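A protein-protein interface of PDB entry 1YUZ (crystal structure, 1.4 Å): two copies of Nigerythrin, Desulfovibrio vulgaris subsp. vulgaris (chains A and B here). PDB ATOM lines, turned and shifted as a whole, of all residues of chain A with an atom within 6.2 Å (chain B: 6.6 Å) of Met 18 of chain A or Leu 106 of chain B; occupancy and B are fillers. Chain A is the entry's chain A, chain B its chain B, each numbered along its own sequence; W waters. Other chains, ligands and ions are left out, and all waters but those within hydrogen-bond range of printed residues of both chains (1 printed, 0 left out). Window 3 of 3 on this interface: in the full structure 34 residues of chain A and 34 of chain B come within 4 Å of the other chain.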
ATOM      1  N   PHE A  16      -6.729 -25.314   6.194  1.00  0.00           N
ATOM      2  CA  PHE A  16      -6.154 -24.044   6.611  1.00  0.00           C
ATOM      3  C   PHE A  16      -7.124 -23.152   7.374  1.00  0.00           C
ATOM      4  O   PHE A  16      -6.847 -21.975   7.593  1.00  0.00           O
ATOM      5  CB  PHE A  16      -5.597 -23.283   5.405  1.00  0.00           C
ATOM      6  CG  PHE A  16      -4.238 -23.756   4.972  1.00  0.00           C
ATOM      7  CD1 PHE A  16      -4.081 -24.991   4.356  1.00  0.00           C
ATOM      8  CD2 PHE A  16      -3.110 -22.978   5.203  1.00  0.00           C
ATOM      9  CE1 PHE A  16      -2.820 -25.447   3.977  1.00  0.00           C
ATOM     10  CE2 PHE A  16      -1.842 -23.427   4.829  1.00  0.00           C
ATOM     11  CZ  PHE A  16      -1.701 -24.664   4.215  1.00  0.00           C
ATOM     12  N   ASN A  17      -8.263 -23.708   7.775  1.00  0.00           N
ATOM     13  CA  ASN A  17      -9.229 -22.930   8.535  1.00  0.00           C
ATOM     14  C   ASN A  17      -8.691 -22.771   9.946  1.00  0.00           C
ATOM     15  O   ASN A  17      -8.031 -23.668  10.473  1.00  0.00           O
ATOM     16  CB  ASN A  17     -10.585 -23.641   8.576  1.00  0.00           C
ATOM     17  CG  ASN A  17     -11.253 -23.687   7.222  1.00  0.00           C
ATOM     18  OD1 ASN A  17     -11.416 -22.658   6.569  1.00  0.00           O
ATOM     19  ND2 ASN A  17     -11.648 -24.879   6.792  1.00  0.00           N
ATOM     20  N   MET A  18      -8.963 -21.628  10.561  1.00  0.00           N
ATOM     21  CA  MET A  18      -8.499 -21.401  11.919  1.00  0.00           C
ATOM     22  C   MET A  18      -9.645 -21.640  12.886  1.00  0.00           C
ATOM     23  O   MET A  18     -10.812 -21.450  12.539  1.00  0.00           O
ATOM     24  CB  MET A  18      -7.984 -19.972  12.087  1.00  0.00           C
ATOM     25  CG  MET A  18      -9.071 -18.914  12.076  1.00  0.00           C
ATOM     26  SD  MET A  18      -8.400 -17.270  12.339  1.00  0.00           S
ATOM     27  CE  MET A  18      -7.745 -16.924  10.692  1.00  0.00           C
ATOM     28  N   VAL A  19      -9.305 -22.061  14.097  1.00  0.00           N
ATOM     29  CA  VAL A  19     -10.307 -22.316  15.123  1.00  0.00           C
ATOM     30  C   VAL A  19     -11.043 -21.026  15.464  1.00  0.00           C
ATOM     31  O   VAL A  19     -10.455 -19.943  15.451  1.00  0.00           O
ATOM     32  CB  VAL A  19      -9.663 -22.886  16.400  1.00  0.00           C
ATOM     33  CG1 VAL A  19      -9.019 -24.228  16.094  1.00  0.00           C
ATOM     34  CG2 VAL A  19      -8.632 -21.914  16.949  1.00  0.00           C
ATOM     35  N   ALA A  20     -12.333 -21.152  15.762  1.00  0.00           N
ATOM     36  CA  ALA A  20     -13.167 -20.003  16.097  1.00  0.00           C
ATOM     37  C   ALA A  20     -12.741 -19.349  17.407  1.00  0.00           C
ATOM     38  O   ALA A  20     -12.658 -18.124  17.499  1.00  0.00           O
ATOM     39  CB  ALA A  20     -14.624 -20.432  16.177  1.00  0.00           C
ATOM     40  N   SER A  22      -9.960 -18.677  19.044  1.00  0.00           N
ATOM     41  CA  SER A  22      -8.513 -18.537  18.971  1.00  0.00           C
ATOM     42  C   SER A  22      -7.861 -18.079  20.269  1.00  0.00           C
ATOM     43  O   SER A  22      -8.417 -17.269  21.012  1.00  0.00           O
ATOM     44  CB  SER A  22      -8.141 -17.564  17.854  1.00  0.00           C
ATOM     45  OG  SER A  22      -6.738 -17.383  17.795  1.00  0.00           O
ATOM     46  N   SER A 120      -3.534 -25.352  13.730  1.00  0.00           N
ATOM     47  CA  SER A 120      -4.952 -25.027  13.581  1.00  0.00           C
ATOM     48  C   SER A 120      -5.389 -23.671  14.116  1.00  0.00           C
ATOM     49  O   SER A 120      -6.505 -23.226  13.842  1.00  0.00           O
ATOM     50  CB  SER A 120      -5.797 -26.110  14.258  1.00  0.00           C
ATOM     51  OG  SER A 120      -5.687 -26.028  15.668  1.00  0.00           O
ATOM     52  N   ASP A 121      -4.516 -23.018  14.872  1.00  0.00           N
ATOM     53  CA  ASP A 121      -4.842 -21.730  15.466  1.00  0.00           C
ATOM     54  C   ASP A 121      -3.837 -20.655  15.071  1.00  0.00           C
ATOM     55  O   ASP A 121      -4.130 -19.797  14.239  1.00  0.00           O
ATOM     56  CB  ASP A 121      -4.885 -21.877  16.994  1.00  0.00           C
ATOM     57  CG  ASP A 121      -5.430 -20.643  17.697  1.00  0.00           C
ATOM     58  OD1 ASP A 121      -5.326 -19.530  17.141  1.00  0.00           O
ATOM     59  OD2 ASP A 121      -5.947 -20.792  18.826  1.00  0.00           O
ATOM     60  N   PRO A 124      -2.602 -20.543  11.064  1.00  0.00           N
ATOM     61  CA  PRO A 124      -3.680 -20.132  10.159  1.00  0.00           C
ATOM     62  C   PRO A 124      -4.038 -18.658  10.378  1.00  0.00           C
ATOM     63  O   PRO A 124      -4.291 -17.923   9.422  1.00  0.00           O
ATOM     64  CB  PRO A 124      -4.822 -21.067  10.545  1.00  0.00           C
ATOM     65  CG  PRO A 124      -4.093 -22.326  10.869  1.00  0.00           C
ATOM     66  CD  PRO A 124      -2.924 -21.831  11.707  1.00  0.00           C
ATOM     67  N   ALA A 125      -4.052 -18.225  11.635  1.00  0.00           N
ATOM     68  CA  ALA A 125      -4.374 -16.832  11.942  1.00  0.00           C
ATOM     69  C   ALA A 125      -3.338 -15.906  11.313  1.00  0.00           C
ATOM     70  O   ALA A 125      -3.679 -14.887  10.709  1.00  0.00           O
ATOM     71  CB  ALA A 125      -4.414 -16.618  13.448  1.00  0.00           C
ATOM     72  N   PHE A 126      -2.067 -16.264  11.456  1.00  0.00           N
ATOM     73  CA  PHE A 126      -0.989 -15.457  10.897  1.00  0.00           C
ATOM     74  C   PHE A 126      -0.999 -15.467   9.374  1.00  0.00           C
ATOM     75  O   PHE A 126      -0.686 -14.458   8.742  1.00  0.00           O
ATOM     76  CB  PHE A 126       0.364 -15.948  11.417  1.00  0.00           C
ATOM     77  CG  PHE A 126       0.587 -15.683  12.882  1.00  0.00           C
ATOM     78  CD1 PHE A 126       1.708 -16.194  13.519  1.00  0.00           C
ATOM     79  CD2 PHE A 126      -0.304 -14.905  13.619  1.00  0.00           C
ATOM     80  CE1 PHE A 126       1.946 -15.939  14.865  1.00  0.00           C
ATOM     81  CE2 PHE A 126      -0.075 -14.643  14.965  1.00  0.00           C
ATOM     82  CZ  PHE A 126       1.054 -15.161  15.590  1.00  0.00           C
ATOM     83  N   ARG A 128      -3.657 -15.756   7.404  1.00  0.00           N
ATOM     84  CA  ARG A 128      -4.739 -14.892   6.949  1.00  0.00           C
ATOM     85  C   ARG A 128      -4.407 -13.417   7.117  1.00  0.00           C
ATOM     86  O   ARG A 128      -4.745 -12.605   6.257  1.00  0.00           O
ATOM     87  CB  ARG A 128      -6.035 -15.235   7.684  1.00  0.00           C
ATOM     88  CG  ARG A 128      -6.556 -16.634   7.378  1.00  0.00           C
ATOM     89  CD  ARG A 128      -6.724 -16.862   5.880  1.00  0.00           C
ATOM     90  NE  ARG A 128      -7.274 -18.183   5.582  1.00  0.00           N
ATOM     91  CZ  ARG A 128      -7.496 -18.644   4.355  1.00  0.00           C
ATOM     92  NH1 ARG A 128      -7.213 -17.894   3.299  1.00  0.00           N
ATOM     93  NH2 ARG A 128      -8.006 -19.857   4.185  1.00  0.00           N
ATOM     94  N   LYS A 129      -3.738 -13.064   8.209  1.00  0.00           N
ATOM     95  CA  LYS A 129      -3.378 -11.670   8.427  1.00  0.00           C
ATOM     96  C   LYS A 129      -2.344 -11.250   7.390  1.00  0.00           C
ATOM     97  O   LYS A 129      -2.369 -10.122   6.902  1.00  0.00           O
ATOM     98  CB  LYS A 129      -2.824 -11.459   9.839  1.00  0.00           C
ATOM     99  CG  LYS A 129      -2.541  -9.996  10.184  1.00  0.00           C
ATOM    100  CD  LYS A 129      -3.789  -9.130  10.010  1.00  0.00           C
ATOM    101  CE  LYS A 129      -3.526  -7.677  10.385  1.00  0.00           C
ATOM    102  NZ  LYS A 129      -3.316  -7.512  11.847  1.00  0.00           N
ATOM    103  N   PHE B  50     -20.295 -34.874  12.799  1.00  0.00           N
ATOM    104  CA  PHE B  50     -19.113 -34.622  11.978  1.00  0.00           C
ATOM    105  C   PHE B  50     -19.127 -35.485  10.714  1.00  0.00           C
ATOM    106  O   PHE B  50     -18.730 -35.034   9.640  1.00  0.00           O
ATOM    107  CB  PHE B  50     -17.837 -34.917  12.771  1.00  0.00           C
ATOM    108  CG  PHE B  50     -17.495 -33.880  13.812  1.00  0.00           C
ATOM    109  CD1 PHE B  50     -16.367 -34.046  14.607  1.00  0.00           C
ATOM    110  CD2 PHE B  50     -18.271 -32.735  13.987  1.00  0.00           C
ATOM    111  CE1 PHE B  50     -16.011 -33.093  15.557  1.00  0.00           C
ATOM    112  CE2 PHE B  50     -17.917 -31.775  14.940  1.00  0.00           C
ATOM    113  CZ  PHE B  50     -16.786 -31.957  15.724  1.00  0.00           C
ATOM    114  N   TYR B 102     -18.662 -28.151  11.954  1.00  0.00           N
ATOM    115  CA  TYR B 102     -18.134 -27.049  11.163  1.00  0.00           C
ATOM    116  C   TYR B 102     -17.335 -27.597   9.988  1.00  0.00           C
ATOM    117  O   TYR B 102     -17.638 -28.680   9.494  1.00  0.00           O
ATOM    118  CB  TYR B 102     -17.278 -26.143  12.049  1.00  0.00           C
ATOM    119  CG  TYR B 102     -18.040 -25.645  13.257  1.00  0.00           C
ATOM    120  CD1 TYR B 102     -18.036 -26.358  14.453  1.00  0.00           C
ATOM    121  CD2 TYR B 102     -18.808 -24.485  13.187  1.00  0.00           C
ATOM    122  CE1 TYR B 102     -18.780 -25.928  15.551  1.00  0.00           C
ATOM    123  CE2 TYR B 102     -19.556 -24.048  14.276  1.00  0.00           C
ATOM    124  CZ  TYR B 102     -19.536 -24.774  15.453  1.00  0.00           C
ATOM    125  OH  TYR B 102     -20.276 -24.347  16.530  1.00  0.00           O
ATOM    126  N   SER B 103     -16.335 -26.856   9.523  1.00  0.00           N
ATOM    127  CA  SER B 103     -15.532 -27.338   8.408  1.00  0.00           C
ATOM    128  C   SER B 103     -14.861 -28.638   8.819  1.00  0.00           C
ATOM    129  O   SER B 103     -14.467 -28.810   9.975  1.00  0.00           O
ATOM    130  CB  SER B 103     -14.491 -26.299   8.003  1.00  0.00           C
ATOM    131  OG  SER B 103     -15.132 -25.175   7.428  1.00  0.00           O
ATOM    132  N   CYS B 104     -14.731 -29.549   7.864  1.00  0.00           N
ATOM    133  CA  CYS B 104     -14.157 -30.858   8.130  1.00  0.00           C
ATOM    134  C   CYS B 104     -12.808 -30.842   8.834  1.00  0.00           C
ATOM    135  O   CYS B 104     -12.594 -31.608   9.776  1.00  0.00           O
ATOM    136  CB  CYS B 104     -14.054 -31.650   6.830  1.00  0.00           C
ATOM    137  SG  CYS B 104     -13.745 -33.399   7.092  1.00  0.00           S
ATOM    138  N   ASP B 105     -11.899 -29.980   8.391  1.00  0.00           N
ATOM    139  CA  ASP B 105     -10.585 -29.930   9.017  1.00  0.00           C
ATOM    140  C   ASP B 105     -10.689 -29.554  10.490  1.00  0.00           C
ATOM    141  O   ASP B 105     -10.047 -30.172  11.336  1.00  0.00           O
ATOM    142  CB  ASP B 105      -9.645 -28.974   8.249  1.00  0.00           C
ATOM    143  CG  ASP B 105     -10.092 -27.519   8.287  1.00  0.00           C
ATOM    144  OD1 ASP B 105     -11.308 -27.242   8.196  1.00  0.00           O
ATOM    145  OD2 ASP B 105      -9.203 -26.641   8.381  1.00  0.00           O
ATOM    146  N   LEU B 106     -11.522 -28.571  10.806  1.00  0.00           N
ATOM    147  CA  LEU B 106     -11.693 -28.160  12.193  1.00  0.00           C
ATOM    148  C   LEU B 106     -12.384 -29.250  13.008  1.00  0.00           C
ATOM    149  O   LEU B 106     -12.118 -29.398  14.201  1.00  0.00           O
ATOM    150  CB  LEU B 106     -12.481 -26.851  12.268  1.00  0.00           C
ATOM    151  CG  LEU B 106     -11.723 -25.635  11.726  1.00  0.00           C
ATOM    152  CD1 LEU B 106     -12.603 -24.406  11.824  1.00  0.00           C
ATOM    153  CD2 LEU B 106     -10.439 -25.434  12.509  1.00  0.00           C
ATOM    154  N   ASN B 107     -13.259 -30.024  12.372  1.00  0.00           N
ATOM    155  CA  ASN B 107     -13.929 -31.103  13.086  1.00  0.00           C
ATOM    156  C   ASN B 107     -12.902 -32.175  13.439  1.00  0.00           C
ATOM    157  O   ASN B 107     -12.949 -32.754  14.523  1.00  0.00           O
ATOM    158  CB  ASN B 107     -15.055 -31.709  12.248  1.00  0.00           C
ATOM    159  CG  ASN B 107     -16.174 -30.725  11.978  1.00  0.00           C
ATOM    160  OD1 ASN B 107     -16.331 -29.737  12.693  1.00  0.00           O
ATOM    161  ND2 ASN B 107     -16.965 -31.000  10.952  1.00  0.00           N
ATOM    162  N   LEU B 108     -11.975 -32.442  12.523  1.00  0.00           N
ATOM    163  CA  LEU B 108     -10.930 -33.422  12.785  1.00  0.00           C
ATOM    164  C   LEU B 108     -10.066 -32.944  13.949  1.00  0.00           C
ATOM    165  O   LEU B 108      -9.652 -33.739  14.781  1.00  0.00           O
ATOM    166  CB  LEU B 108     -10.062 -33.631  11.543  1.00  0.00           C
ATOM    167  CG  LEU B 108     -10.682 -34.482  10.433  1.00  0.00           C
ATOM    168  CD1 LEU B 108      -9.844 -34.359   9.171  1.00  0.00           C
ATOM    169  CD2 LEU B 108     -10.767 -35.931  10.878  1.00  0.00           C
ATOM    170  N   ILE B 109      -9.797 -31.642  14.008  1.00  0.00           N
ATOM    171  CA  ILE B 109      -8.998 -31.088  15.098  1.00  0.00           C
ATOM    172  C   ILE B 109      -9.783 -31.180  16.411  1.00  0.00           C
ATOM    173  O   ILE B 109      -9.227 -31.535  17.450  1.00  0.00           O
ATOM    174  CB  ILE B 109      -8.607 -29.614  14.812  1.00  0.00           C
ATOM    175  CG1 ILE B 109      -7.607 -29.558  13.649  1.00  0.00           C
ATOM    176  CG2 ILE B 109      -8.031 -28.968  16.069  1.00  0.00           C
ATOM    177  CD1 ILE B 109      -6.267 -30.238  13.930  1.00  0.00           C
ATOM    178  N   SER B 110     -11.074 -30.867  16.365  1.00  0.00           N
ATOM    179  CA  SER B 110     -11.913 -30.960  17.555  1.00  0.00           C
ATOM    180  C   SER B 110     -11.902 -32.408  18.037  1.00  0.00           C
ATOM    181  O   SER B 110     -11.791 -32.681  19.232  1.00  0.00           O
ATOM    182  CB  SER B 110     -13.342 -30.532  17.220  1.00  0.00           C
ATOM    183  OG  SER B 110     -14.207 -30.720  18.326  1.00  0.00           O
ATOM    184  N   GLY B 111     -12.018 -33.338  17.097  1.00  0.00           N
ATOM    185  CA  GLY B 111     -11.996 -34.742  17.452  1.00  0.00           C
ATOM    186  C   GLY B 111     -10.668 -35.121  18.083  1.00  0.00           C
ATOM    187  O   GLY B 111     -10.633 -35.748  19.140  1.00  0.00           O
ATOM    188  N   TYR B 160      -6.355 -35.463   8.841  1.00  0.00           N
ATOM    189  CA  TYR B 160      -6.211 -34.018   8.707  1.00  0.00           C
ATOM    190  C   TYR B 160      -5.031 -33.705   7.785  1.00  0.00           C
ATOM    191  O   TYR B 160      -5.129 -32.855   6.901  1.00  0.00           O
ATOM    192  CB  TYR B 160      -5.977 -33.405  10.091  1.00  0.00           C
ATOM    193  CG  TYR B 160      -5.786 -31.904  10.120  1.00  0.00           C
ATOM    194  CD1 TYR B 160      -6.874 -31.042  10.262  1.00  0.00           C
ATOM    195  CD2 TYR B 160      -4.508 -31.348  10.075  1.00  0.00           C
ATOM    196  CE1 TYR B 160      -6.691 -29.667  10.372  1.00  0.00           C
ATOM    197  CE2 TYR B 160      -4.315 -29.975  10.181  1.00  0.00           C
ATOM    198  CZ  TYR B 160      -5.411 -29.145  10.334  1.00  0.00           C
ATOM    199  OH  TYR B 160      -5.216 -27.795  10.486  1.00  0.00           O
ATOM    200  N   ILE B 163      -6.045 -34.552   4.273  1.00  0.00           N
ATOM    201  CA  ILE B 163      -7.410 -34.146   3.977  1.00  0.00           C
ATOM    202  C   ILE B 163      -7.696 -34.017   2.481  1.00  0.00           C
ATOM    203  O   ILE B 163      -8.812 -34.279   2.039  1.00  0.00           O
ATOM    204  CB  ILE B 163      -7.764 -32.823   4.704  1.00  0.00           C
ATOM    205  CG1 ILE B 163      -9.268 -32.565   4.605  1.00  0.00           C
ATOM    206  CG2 ILE B 163      -6.975 -31.665   4.112  1.00  0.00           C
ATOM    207  CD1 ILE B 163      -9.776 -31.521   5.577  1.00  0.00           C
HETATM  208  O   HOH W   1      -7.472 -26.394  10.449  1.00  0.00           O
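No position is printed for both chains.
Of the 13 printed residues of chain A, 5 touch a printed residue of chain B. Among the printed residues, 7 pairs touch across the chains. Among the printed residues, no Asp or Glu carboxylate lies within 4 Å of a Lys or Arg side-chain nitrogen of the other chain.
Water W1 lies within hydrogen-bond range of OH of Tyr 160 of chain B (2.7 Å), OD2 of Asp 105 of chain B (2.7 Å) and O of Asn 17 of chain A (2.8 Å).
The backbone NH (N) of Val 19 of chain A is in hydrogen-bond range of the backbone carbonyl oxygen (O) of Ser 120 of chain A, 3.0 Å away. The side-chain amide oxygen (OD1) of Asn 107 of chain B lies close to the backbone carbonyl oxygen (O) of Ser 103 of chain B, at 3.4 Å.
ND2 of Asn 17 of chain A lies within hydrogen-bond range of OD1 of Asp 105 of chain B.
Of the printed residues of chain B, Met 18 of chain A touches Leu 106. Printed residues of chain A within 4 Å of Leu 106 of chain B: Asn 17, Met 18 and Val 19. Of the printed residues of chain B, Phe 16 of chain A touches Asp 105. Of the printed residues of chain B, Val 19 of chain A touches Leu 106. Of the printed residues of chain B, Ser 120 of chain A touches Ile 109. Arg 128 of chain A touches none of the printed residues of chain B. Phe 126 of chain A touches none of the printed residues of chain B. The nearest printed residue of chain B that does not touch Met 18 of chain A is Asp 105 of chain B (5.5 Å). The nearest printed residue of chain A that does not touch Leu 106 of chain B is Ser 120 of chain A (4.7 Å).
Among the printed residues, pairs that only touch across the chains: Asn 17 of chain A with Ser 103 of chain B (3.4 Å), Met 18 of chain A with Leu 106 of chain B (3.5 Å), Phe 16 of chain A with Asp 105 of chain B (3.6 Å), Asn 17 of chain A with Leu 106 of chain B (3.6 Å), Ser 120 of chain A with Ile 109 of chain B (3.8 Å) and Val 19 of chain A with Leu 106 of chain B (3.9 Å).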
